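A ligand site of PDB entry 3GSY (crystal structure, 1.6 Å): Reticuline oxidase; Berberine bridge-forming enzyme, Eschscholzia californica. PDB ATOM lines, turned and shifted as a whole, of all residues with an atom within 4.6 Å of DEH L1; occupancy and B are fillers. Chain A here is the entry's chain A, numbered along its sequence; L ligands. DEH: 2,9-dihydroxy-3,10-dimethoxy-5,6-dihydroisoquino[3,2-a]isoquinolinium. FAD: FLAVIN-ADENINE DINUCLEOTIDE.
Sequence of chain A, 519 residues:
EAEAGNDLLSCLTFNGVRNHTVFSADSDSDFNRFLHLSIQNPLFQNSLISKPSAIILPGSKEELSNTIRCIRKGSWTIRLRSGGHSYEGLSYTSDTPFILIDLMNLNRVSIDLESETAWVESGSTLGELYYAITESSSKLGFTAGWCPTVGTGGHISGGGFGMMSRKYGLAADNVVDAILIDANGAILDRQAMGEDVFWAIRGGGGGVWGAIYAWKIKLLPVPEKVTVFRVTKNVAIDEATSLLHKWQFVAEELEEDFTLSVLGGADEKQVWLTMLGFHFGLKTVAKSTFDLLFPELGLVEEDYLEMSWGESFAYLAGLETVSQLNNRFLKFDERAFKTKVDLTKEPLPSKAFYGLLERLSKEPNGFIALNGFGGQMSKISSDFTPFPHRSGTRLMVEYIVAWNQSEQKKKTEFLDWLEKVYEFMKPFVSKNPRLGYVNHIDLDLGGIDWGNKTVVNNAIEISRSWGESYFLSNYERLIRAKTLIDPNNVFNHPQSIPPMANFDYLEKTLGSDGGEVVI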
ATOM      1  N   TYR A  87      17.114  -0.786   6.788  1.00  0.00           N
ATOM      2  CA  TYR A  87      18.248  -1.525   6.236  1.00  0.00           C
ATOM      3  C   TYR A  87      19.589  -0.882   6.597  1.00  0.00           C
ATOM      4  O   TYR A  87      20.607  -1.573   6.632  1.00  0.00           O
ATOM      5  CB  TYR A  87      18.140  -1.652   4.711  1.00  0.00           C
ATOM      6  CG  TYR A  87      16.984  -2.503   4.233  1.00  0.00           C
ATOM      7  CD1 TYR A  87      16.377  -3.430   5.078  1.00  0.00           C
ATOM      8  CD2 TYR A  87      16.543  -2.419   2.924  1.00  0.00           C
ATOM      9  CE1 TYR A  87      15.328  -4.218   4.624  1.00  0.00           C
ATOM     10  CE2 TYR A  87      15.518  -3.192   2.466  1.00  0.00           C
ATOM     11  CZ  TYR A  87      14.916  -4.099   3.320  1.00  0.00           C
ATOM     12  OH  TYR A  87      13.870  -4.870   2.844  1.00  0.00           O
ATOM     13  N   TRP A 146       5.599  -8.515   3.675  1.00  0.00           N
ATOM     14  CA  TRP A 146       5.677  -9.945   3.930  1.00  0.00           C
ATOM     15  C   TRP A 146       6.303 -10.244   5.307  1.00  0.00           C
ATOM     16  O   TRP A 146       5.872 -11.179   5.997  1.00  0.00           O
ATOM     17  CB  TRP A 146       6.493 -10.540   2.772  1.00  0.00           C
ATOM     18  CG  TRP A 146       6.764 -12.007   2.747  1.00  0.00           C
ATOM     19  CD1 TRP A 146       5.929 -13.002   2.307  1.00  0.00           C
ATOM     20  CD2 TRP A 146       7.996 -12.648   3.109  1.00  0.00           C
ATOM     21  NE1 TRP A 146       6.560 -14.225   2.396  1.00  0.00           N
ATOM     22  CE2 TRP A 146       7.826 -14.034   2.892  1.00  0.00           C
ATOM     23  CE3 TRP A 146       9.213 -12.183   3.625  1.00  0.00           C
ATOM     24  CZ2 TRP A 146       8.835 -14.957   3.159  1.00  0.00           C
ATOM     25  CZ3 TRP A 146      10.217 -13.112   3.886  1.00  0.00           C
ATOM     26  CH2 TRP A 146      10.019 -14.483   3.661  1.00  0.00           C
ATOM     27  N   CYS A 147       7.280  -9.435   5.717  1.00  0.00           N
ATOM     28  CA  CYS A 147       7.966  -9.654   7.000  1.00  0.00           C
ATOM     29  C   CYS A 147       7.118  -9.172   8.191  1.00  0.00           C
ATOM     30  O   CYS A 147       6.793  -7.992   8.305  1.00  0.00           O
ATOM     31  CB  CYS A 147       9.336  -8.942   7.026  1.00  0.00           C
ATOM     32  SG  CYS A 147      10.536  -9.373   5.733  1.00  0.00           S
ATOM     33  N   MET A 163       2.332  -9.276  -0.837  1.00  0.00           N
ATOM     34  CA  MET A 163       1.732 -10.329  -1.643  1.00  0.00           C
ATOM     35  C   MET A 163       0.349  -9.997  -2.189  1.00  0.00           C
ATOM     36  O   MET A 163      -0.126 -10.667  -3.100  1.00  0.00           O
ATOM     37  CB  MET A 163       1.681 -11.640  -0.853  1.00  0.00           C
ATOM     38  CG  MET A 163       3.032 -12.278  -0.588  1.00  0.00           C
ATOM     39  SD  MET A 163       3.843 -12.906  -2.076  1.00  0.00           S
ATOM     40  CE  MET A 163       2.787 -14.277  -2.560  1.00  0.00           C
ATOM     41  N   SER A 261       5.515 -15.103  -6.572  1.00  0.00           N
ATOM     42  CA  SER A 261       6.816 -14.512  -6.294  1.00  0.00           C
ATOM     43  C   SER A 261       7.867 -15.591  -6.032  1.00  0.00           C
ATOM     44  O   SER A 261       7.547 -16.774  -5.876  1.00  0.00           O
ATOM     45  CB  SER A 261       6.687 -13.552  -5.107  1.00  0.00           C
ATOM     46  OG  SER A 261       5.768 -12.520  -5.422  1.00  0.00           O
ATOM     47  N   LEU A 263      11.719 -16.665  -4.027  1.00  0.00           N
ATOM     48  CA  LEU A 263      12.957 -16.506  -3.294  1.00  0.00           C
ATOM     49  C   LEU A 263      13.939 -17.505  -3.889  1.00  0.00           C
ATOM     50  O   LEU A 263      13.590 -18.661  -4.125  1.00  0.00           O
ATOM     51  CB  LEU A 263      12.745 -16.799  -1.812  1.00  0.00           C
ATOM     52  CG  LEU A 263      11.976 -15.761  -1.000  1.00  0.00           C
ATOM     53  CD1 LEU A 263      11.397 -16.423   0.248  1.00  0.00           C
ATOM     54  CD2 LEU A 263      12.893 -14.595  -0.633  1.00  0.00           C
ATOM     55  N   LEU A 276       6.382 -18.738  -4.216  1.00  0.00           N
ATOM     56  CA  LEU A 276       5.338 -18.272  -3.302  1.00  0.00           C
ATOM     57  C   LEU A 276       4.103 -17.871  -4.081  1.00  0.00           C
ATOM     58  O   LEU A 276       4.124 -16.901  -4.851  1.00  0.00           O
ATOM     59  CB  LEU A 276       5.838 -17.086  -2.478  1.00  0.00           C
ATOM     60  CG  LEU A 276       7.122 -17.277  -1.661  1.00  0.00           C
ATOM     61  CD1 LEU A 276       7.561 -15.939  -1.076  1.00  0.00           C
ATOM     62  CD2 LEU A 276       6.922 -18.301  -0.575  1.00  0.00           C
ATOM     63  N   PHE A 332      12.825 -13.294  13.359  1.00  0.00           N
ATOM     64  CA  PHE A 332      12.493 -13.726  12.014  1.00  0.00           C
ATOM     65  C   PHE A 332      13.749 -14.165  11.260  1.00  0.00           C
ATOM     66  O   PHE A 332      13.773 -15.221  10.616  1.00  0.00           O
ATOM     67  CB  PHE A 332      11.793 -12.598  11.264  1.00  0.00           C
ATOM     68  CG  PHE A 332      11.185 -13.027   9.961  1.00  0.00           C
ATOM     69  CD1 PHE A 332      11.668 -12.532   8.760  1.00  0.00           C
ATOM     70  CD2 PHE A 332      10.123 -13.927   9.927  1.00  0.00           C
ATOM     71  CE1 PHE A 332      11.115 -12.918   7.551  1.00  0.00           C
ATOM     72  CE2 PHE A 332       9.551 -14.322   8.728  1.00  0.00           C
ATOM     73  CZ  PHE A 332      10.057 -13.820   7.535  1.00  0.00           C
ATOM     74  N   ASP A 333      14.795 -13.345  11.345  1.00  0.00           N
ATOM     75  CA  ASP A 333      16.074 -13.655  10.727  1.00  0.00           C
ATOM     76  C   ASP A 333      17.165 -12.900  11.479  1.00  0.00           C
ATOM     77  O   ASP A 333      17.272 -11.678  11.372  1.00  0.00           O
ATOM     78  CB  ASP A 333      16.055 -13.257   9.237  1.00  0.00           C
ATOM     79  CG  ASP A 333      17.215 -13.871   8.451  1.00  0.00           C
ATOM     80  OD1 ASP A 333      18.227 -14.241   9.070  1.00  0.00           O
ATOM     81  OD2 ASP A 333      17.099 -13.980   7.215  1.00  0.00           O
ATOM     82  N   PHE A 337      22.995  -8.178   7.567  1.00  0.00           N
ATOM     83  CA  PHE A 337      22.758  -8.243   6.128  1.00  0.00           C
ATOM     84  C   PHE A 337      22.929  -6.923   5.429  1.00  0.00           C
ATOM     85  O   PHE A 337      22.913  -5.848   6.043  1.00  0.00           O
ATOM     86  CB  PHE A 337      21.358  -8.814   5.848  1.00  0.00           C
ATOM     87  CG  PHE A 337      20.229  -7.880   6.212  1.00  0.00           C
ATOM     88  CD1 PHE A 337      19.676  -7.031   5.247  1.00  0.00           C
ATOM     89  CD2 PHE A 337      19.720  -7.846   7.498  1.00  0.00           C
ATOM     90  CE1 PHE A 337      18.631  -6.169   5.578  1.00  0.00           C
ATOM     91  CE2 PHE A 337      18.675  -6.993   7.839  1.00  0.00           C
ATOM     92  CZ  PHE A 337      18.134  -6.150   6.870  1.00  0.00           C
ATOM     93  N   PHE A 367      21.037 -14.361  -1.559  1.00  0.00           N
ATOM     94  CA  PHE A 367      19.784 -14.811  -2.130  1.00  0.00           C
ATOM     95  C   PHE A 367      19.069 -13.662  -2.836  1.00  0.00           C
ATOM     96  O   PHE A 367      19.449 -12.511  -2.693  1.00  0.00           O
ATOM     97  CB  PHE A 367      18.889 -15.541  -1.112  1.00  0.00           C
ATOM     98  CG  PHE A 367      18.398 -14.680   0.028  1.00  0.00           C
ATOM     99  CD1 PHE A 367      17.119 -14.122  -0.003  1.00  0.00           C
ATOM    100  CD2 PHE A 367      19.191 -14.462   1.147  1.00  0.00           C
ATOM    101  CE1 PHE A 367      16.653 -13.356   1.061  1.00  0.00           C
ATOM    102  CE2 PHE A 367      18.731 -13.681   2.205  1.00  0.00           C
ATOM    103  CZ  PHE A 367      17.471 -13.128   2.163  1.00  0.00           C
ATOM    104  N   ALA A 369      15.077 -12.027  -4.118  1.00  0.00           N
ATOM    105  CA  ALA A 369      13.629 -12.047  -3.997  1.00  0.00           C
ATOM    106  C   ALA A 369      13.057 -11.345  -5.203  1.00  0.00           C
ATOM    107  O   ALA A 369      13.459 -10.222  -5.512  1.00  0.00           O
ATOM    108  CB  ALA A 369      13.177 -11.368  -2.709  1.00  0.00           C
ATOM    109  N   ASN A 371       9.617 -10.117  -7.413  1.00  0.00           N
ATOM    110  CA  ASN A 371       8.199  -9.804  -7.446  1.00  0.00           C
ATOM    111  C   ASN A 371       7.799  -9.155  -8.754  1.00  0.00           C
ATOM    112  O   ASN A 371       8.518  -8.298  -9.289  1.00  0.00           O
ATOM    113  CB  ASN A 371       7.849  -8.810  -6.322  1.00  0.00           C
ATOM    114  CG  ASN A 371       7.674  -9.486  -4.995  1.00  0.00           C
ATOM    115  OD1 ASN A 371       6.626 -10.075  -4.735  1.00  0.00           O
ATOM    116  ND2 ASN A 371       8.687  -9.395  -4.134  1.00  0.00           N
ATOM    117  N   GLU A 398      15.263  -7.998  -5.620  1.00  0.00           N
ATOM    118  CA  GLU A 398      16.080  -7.710  -4.442  1.00  0.00           C
ATOM    119  C   GLU A 398      17.247  -8.667  -4.391  1.00  0.00           C
ATOM    120  O   GLU A 398      17.072  -9.866  -4.619  1.00  0.00           O
ATOM    121  CB  GLU A 398      15.248  -7.836  -3.170  1.00  0.00           C
ATOM    122  CG  GLU A 398      13.982  -6.999  -3.154  1.00  0.00           C
ATOM    123  CD  GLU A 398      13.094  -7.306  -1.962  1.00  0.00           C
ATOM    124  OE1 GLU A 398      13.595  -7.261  -0.818  1.00  0.00           O
ATOM    125  OE2 GLU A 398      11.890  -7.585  -2.168  1.00  0.00           O
ATOM    126  N   ILE A 400      20.214  -9.929  -1.755  1.00  0.00           N
ATOM    127  CA  ILE A 400      20.575  -9.888  -0.334  1.00  0.00           C
ATOM    128  C   ILE A 400      21.779 -10.777  -0.040  1.00  0.00           C
ATOM    129  O   ILE A 400      21.910 -11.869  -0.585  1.00  0.00           O
ATOM    130  CB  ILE A 400      19.396 -10.386   0.547  1.00  0.00           C
ATOM    131  CG1 ILE A 400      18.107  -9.632   0.236  1.00  0.00           C
ATOM    132  CG2 ILE A 400      19.746 -10.290   2.022  1.00  0.00           C
ATOM    133  CD1 ILE A 400      17.264 -10.274  -0.840  1.00  0.00           C
HETATM  134  C2  DEH L   1      13.961 -11.535   3.802  1.00  0.00           C
HETATM  135  C3  DEH L   1      14.911 -11.732   4.797  1.00  0.00           C
HETATM  136  C5  DEH L   1      15.767 -10.732   5.123  1.00  0.00           C
HETATM  137  C8  DEH L   1      15.694  -9.468   4.430  1.00  0.00           C
HETATM  138  C9  DEH L   1      14.733  -9.293   3.435  1.00  0.00           C
HETATM  139  C10 DEH L   1      14.613  -7.984   2.683  1.00  0.00           C
HETATM  140  C11 DEH L   1      13.098  -7.618   2.310  1.00  0.00           C
HETATM  141  N12 DEH L   1      12.410  -8.833   1.785  1.00  0.00           N
HETATM  142  C14 DEH L   1      12.899 -10.123   2.099  1.00  0.00           C
HETATM  143  C16 DEH L   1      12.256 -11.270   1.598  1.00  0.00           C
HETATM  144  C17 DEH L   1      11.159 -11.133   0.825  1.00  0.00           C
HETATM  145  C25 DEH L   1      10.502 -12.282   0.338  1.00  0.00           C
HETATM  146  C24 DEH L   1       9.395 -12.131  -0.441  1.00  0.00           C
HETATM  147  C21 DEH L   1       8.915 -10.851  -0.735  1.00  0.00           C
HETATM  148  O22 DEH L   1       7.818 -10.701  -1.505  1.00  0.00           O
HETATM  149  C23 DEH L   1       7.130 -11.876  -1.970  1.00  0.00           C
HETATM  150  C19 DEH L   1       9.565  -9.717  -0.243  1.00  0.00           C
HETATM  151  O20 DEH L   1       9.085  -8.460  -0.529  1.00  0.00           O
HETATM  152  C18 DEH L   1      10.662  -9.868   0.527  1.00  0.00           C
HETATM  153  C1  DEH L   1      13.880 -10.304   3.137  1.00  0.00           C
HETATM  154  C13 DEH L   1      11.329  -8.692   1.027  1.00  0.00           C
HETATM  155  O6  DEH L   1      16.674 -10.938   6.079  1.00  0.00           O
HETATM  156  C7  DEH L   1      17.869 -10.146   6.127  1.00  0.00           C
HETATM  157  O4  DEH L   1      14.992 -12.949   5.465  1.00  0.00           O
HETATM  158  PA  FAD L   2      12.380   1.722  11.499  1.00  0.00           P
HETATM  159  O1A FAD L   2      13.841   1.394  11.367  1.00  0.00           O
HETATM  160  O2A FAD L   2      11.855   1.852  12.906  1.00  0.00           O
HETATM  161  O5B FAD L   2      12.016   3.052  10.687  1.00  0.00           O
HETATM  162  C5B FAD L   2      12.384   3.245   9.348  1.00  0.00           C
HETATM  163  C4B FAD L   2      12.441   4.752   9.076  1.00  0.00           C
HETATM  164  O4B FAD L   2      11.174   5.330   9.365  1.00  0.00           O
HETATM  165  C3B FAD L   2      13.433   5.483   9.964  1.00  0.00           C
HETATM  166  O3B FAD L   2      13.843   6.643   9.256  1.00  0.00           O
HETATM  167  C2B FAD L   2      12.602   5.900  11.159  1.00  0.00           C
HETATM  168  O2B FAD L   2      13.115   7.006  11.900  1.00  0.00           O
HETATM  169  C1B FAD L   2      11.289   6.220  10.472  1.00  0.00           C
HETATM  170  N9A FAD L   2      10.106   6.026  11.336  1.00  0.00           N
HETATM  171  C8A FAD L   2       9.832   4.958  12.151  1.00  0.00           C
HETATM  172  N7A FAD L   2       8.646   5.191  12.769  1.00  0.00           N
HETATM  173  C5A FAD L   2       8.171   6.396  12.359  1.00  0.00           C
HETATM  174  C6A FAD L   2       7.018   7.116  12.665  1.00  0.00           C
HETATM  175  N6A FAD L   2       6.120   6.641  13.525  1.00  0.00           N
HETATM  176  N1A FAD L   2       6.826   8.341  12.075  1.00  0.00           N
HETATM  177  C2A FAD L   2       7.757   8.851  11.182  1.00  0.00           C
HETATM  178  N3A FAD L   2       8.897   8.137  10.880  1.00  0.00           N
HETATM  179  C4A FAD L   2       9.091   6.921  11.459  1.00  0.00           C
HETATM  180  N1  FAD L   2       9.394  -3.646   2.776  1.00  0.00           N
HETATM  181  C2  FAD L   2       8.329  -3.831   1.908  1.00  0.00           C
HETATM  182  O2  FAD L   2       7.806  -2.870   1.321  1.00  0.00           O
HETATM  183  N3  FAD L   2       7.824  -5.108   1.742  1.00  0.00           N
HETATM  184  C4  FAD L   2       8.355  -6.172   2.437  1.00  0.00           C
HETATM  185  O4  FAD L   2       7.858  -7.301   2.238  1.00  0.00           O
HETATM  186  C4X FAD L   2       9.451  -5.977   3.281  1.00  0.00           C
HETATM  187  N5  FAD L   2       9.981  -7.023   4.045  1.00  0.00           N
HETATM  188  C5X FAD L   2      10.933  -6.785   5.011  1.00  0.00           C
HETATM  189  C6  FAD L   2      11.428  -7.841   5.784  1.00  0.00           C
HETATM  190  C7  FAD L   2      12.345  -7.604   6.801  1.00  0.00           C
HETATM  191  C7M FAD L   2      12.873  -8.771   7.595  1.00  0.00           C
HETATM  192  C8  FAD L   2      12.796  -6.313   7.056  1.00  0.00           C
HETATM  193  C8M FAD L   2      13.732  -6.033   8.202  1.00  0.00           C
HETATM  194  C9  FAD L   2      12.352  -5.270   6.232  1.00  0.00           C
HETATM  195  C9A FAD L   2      11.429  -5.499   5.211  1.00  0.00           C
HETATM  196  N10 FAD L   2      11.030  -4.497   4.339  1.00  0.00           N
HETATM  197  C10 FAD L   2       9.972  -4.708   3.459  1.00  0.00           C
HETATM  198  C1' FAD L   2      11.609  -3.110   4.455  1.00  0.00           C
HETATM  199  C2' FAD L   2      10.733  -2.261   5.367  1.00  0.00           C
HETATM  200  O2' FAD L   2       9.547  -1.889   4.679  1.00  0.00           O
HETATM  201  C3' FAD L   2      11.467  -0.989   5.768  1.00  0.00           C
HETATM  202  O3' FAD L   2      12.679  -1.347   6.415  1.00  0.00           O
HETATM  203  C4' FAD L   2      10.607  -0.149   6.693  1.00  0.00           C
HETATM  204  O4' FAD L   2      10.876   1.238   6.516  1.00  0.00           O
HETATM  205  C5' FAD L   2      10.842  -0.519   8.161  1.00  0.00           C
HETATM  206  O5' FAD L   2       9.948   0.173   9.017  1.00  0.00           O
HETATM  207  P   FAD L   2      10.174  -0.013  10.588  1.00  0.00           P
HETATM  208  O1P FAD L   2       9.171   0.799  11.359  1.00  0.00           O
HETATM  209  O2P FAD L   2      10.274  -1.475  10.911  1.00  0.00           O
HETATM  210  O3P FAD L   2      11.705   0.501  10.704  1.00  0.00           O
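An oxygen (O20) of DEH L1 is in hydrogen-bond range of the side-chain carboxylate (OE2) of Glu 398 (3.4 Å). ND2 of Asn 371 lies within hydrogen-bond range of O22 of DEH L1 (3.1 Å). SG of Cys 147 is bonded to C6 of FAD L2 (1.8 Å). O4 of FAD L2 sits at hydrogen-bond distance from N of Trp 146, at 2.9 Å. OD2 of Asp 333 lies within hydrogen-bond range of O4 of DEH L1 (2.9 Å).
Merely in contact with DEH L1: Tyr 87, Trp 146, Met 163, Ser 261, Leu 263, Phe 337 and Phe 367. Of the 15 residues printed, 10 come within 4 Å of DEH L1.
The backbone NH (N) of Glu 398 sits at hydrogen-bond distance from the backbone carbonyl oxygen (O) of Ala 369 (2.9 Å). OG of Ser 261 is in hydrogen-bond range of OD1 of Asn 371 (2.7 Å). N of Leu 276 is in hydrogen-bond range of O of Ser 261 (2.8 Å). The backbone NH (N) of Phe 367 sits at hydrogen-bond distance from the backbone carbonyl oxygen (O) of Ile 400 (2.8 Å).
O4 of FAD L2 sits at hydrogen-bond distance from O20 of DEH L1, 3.2 Å away.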
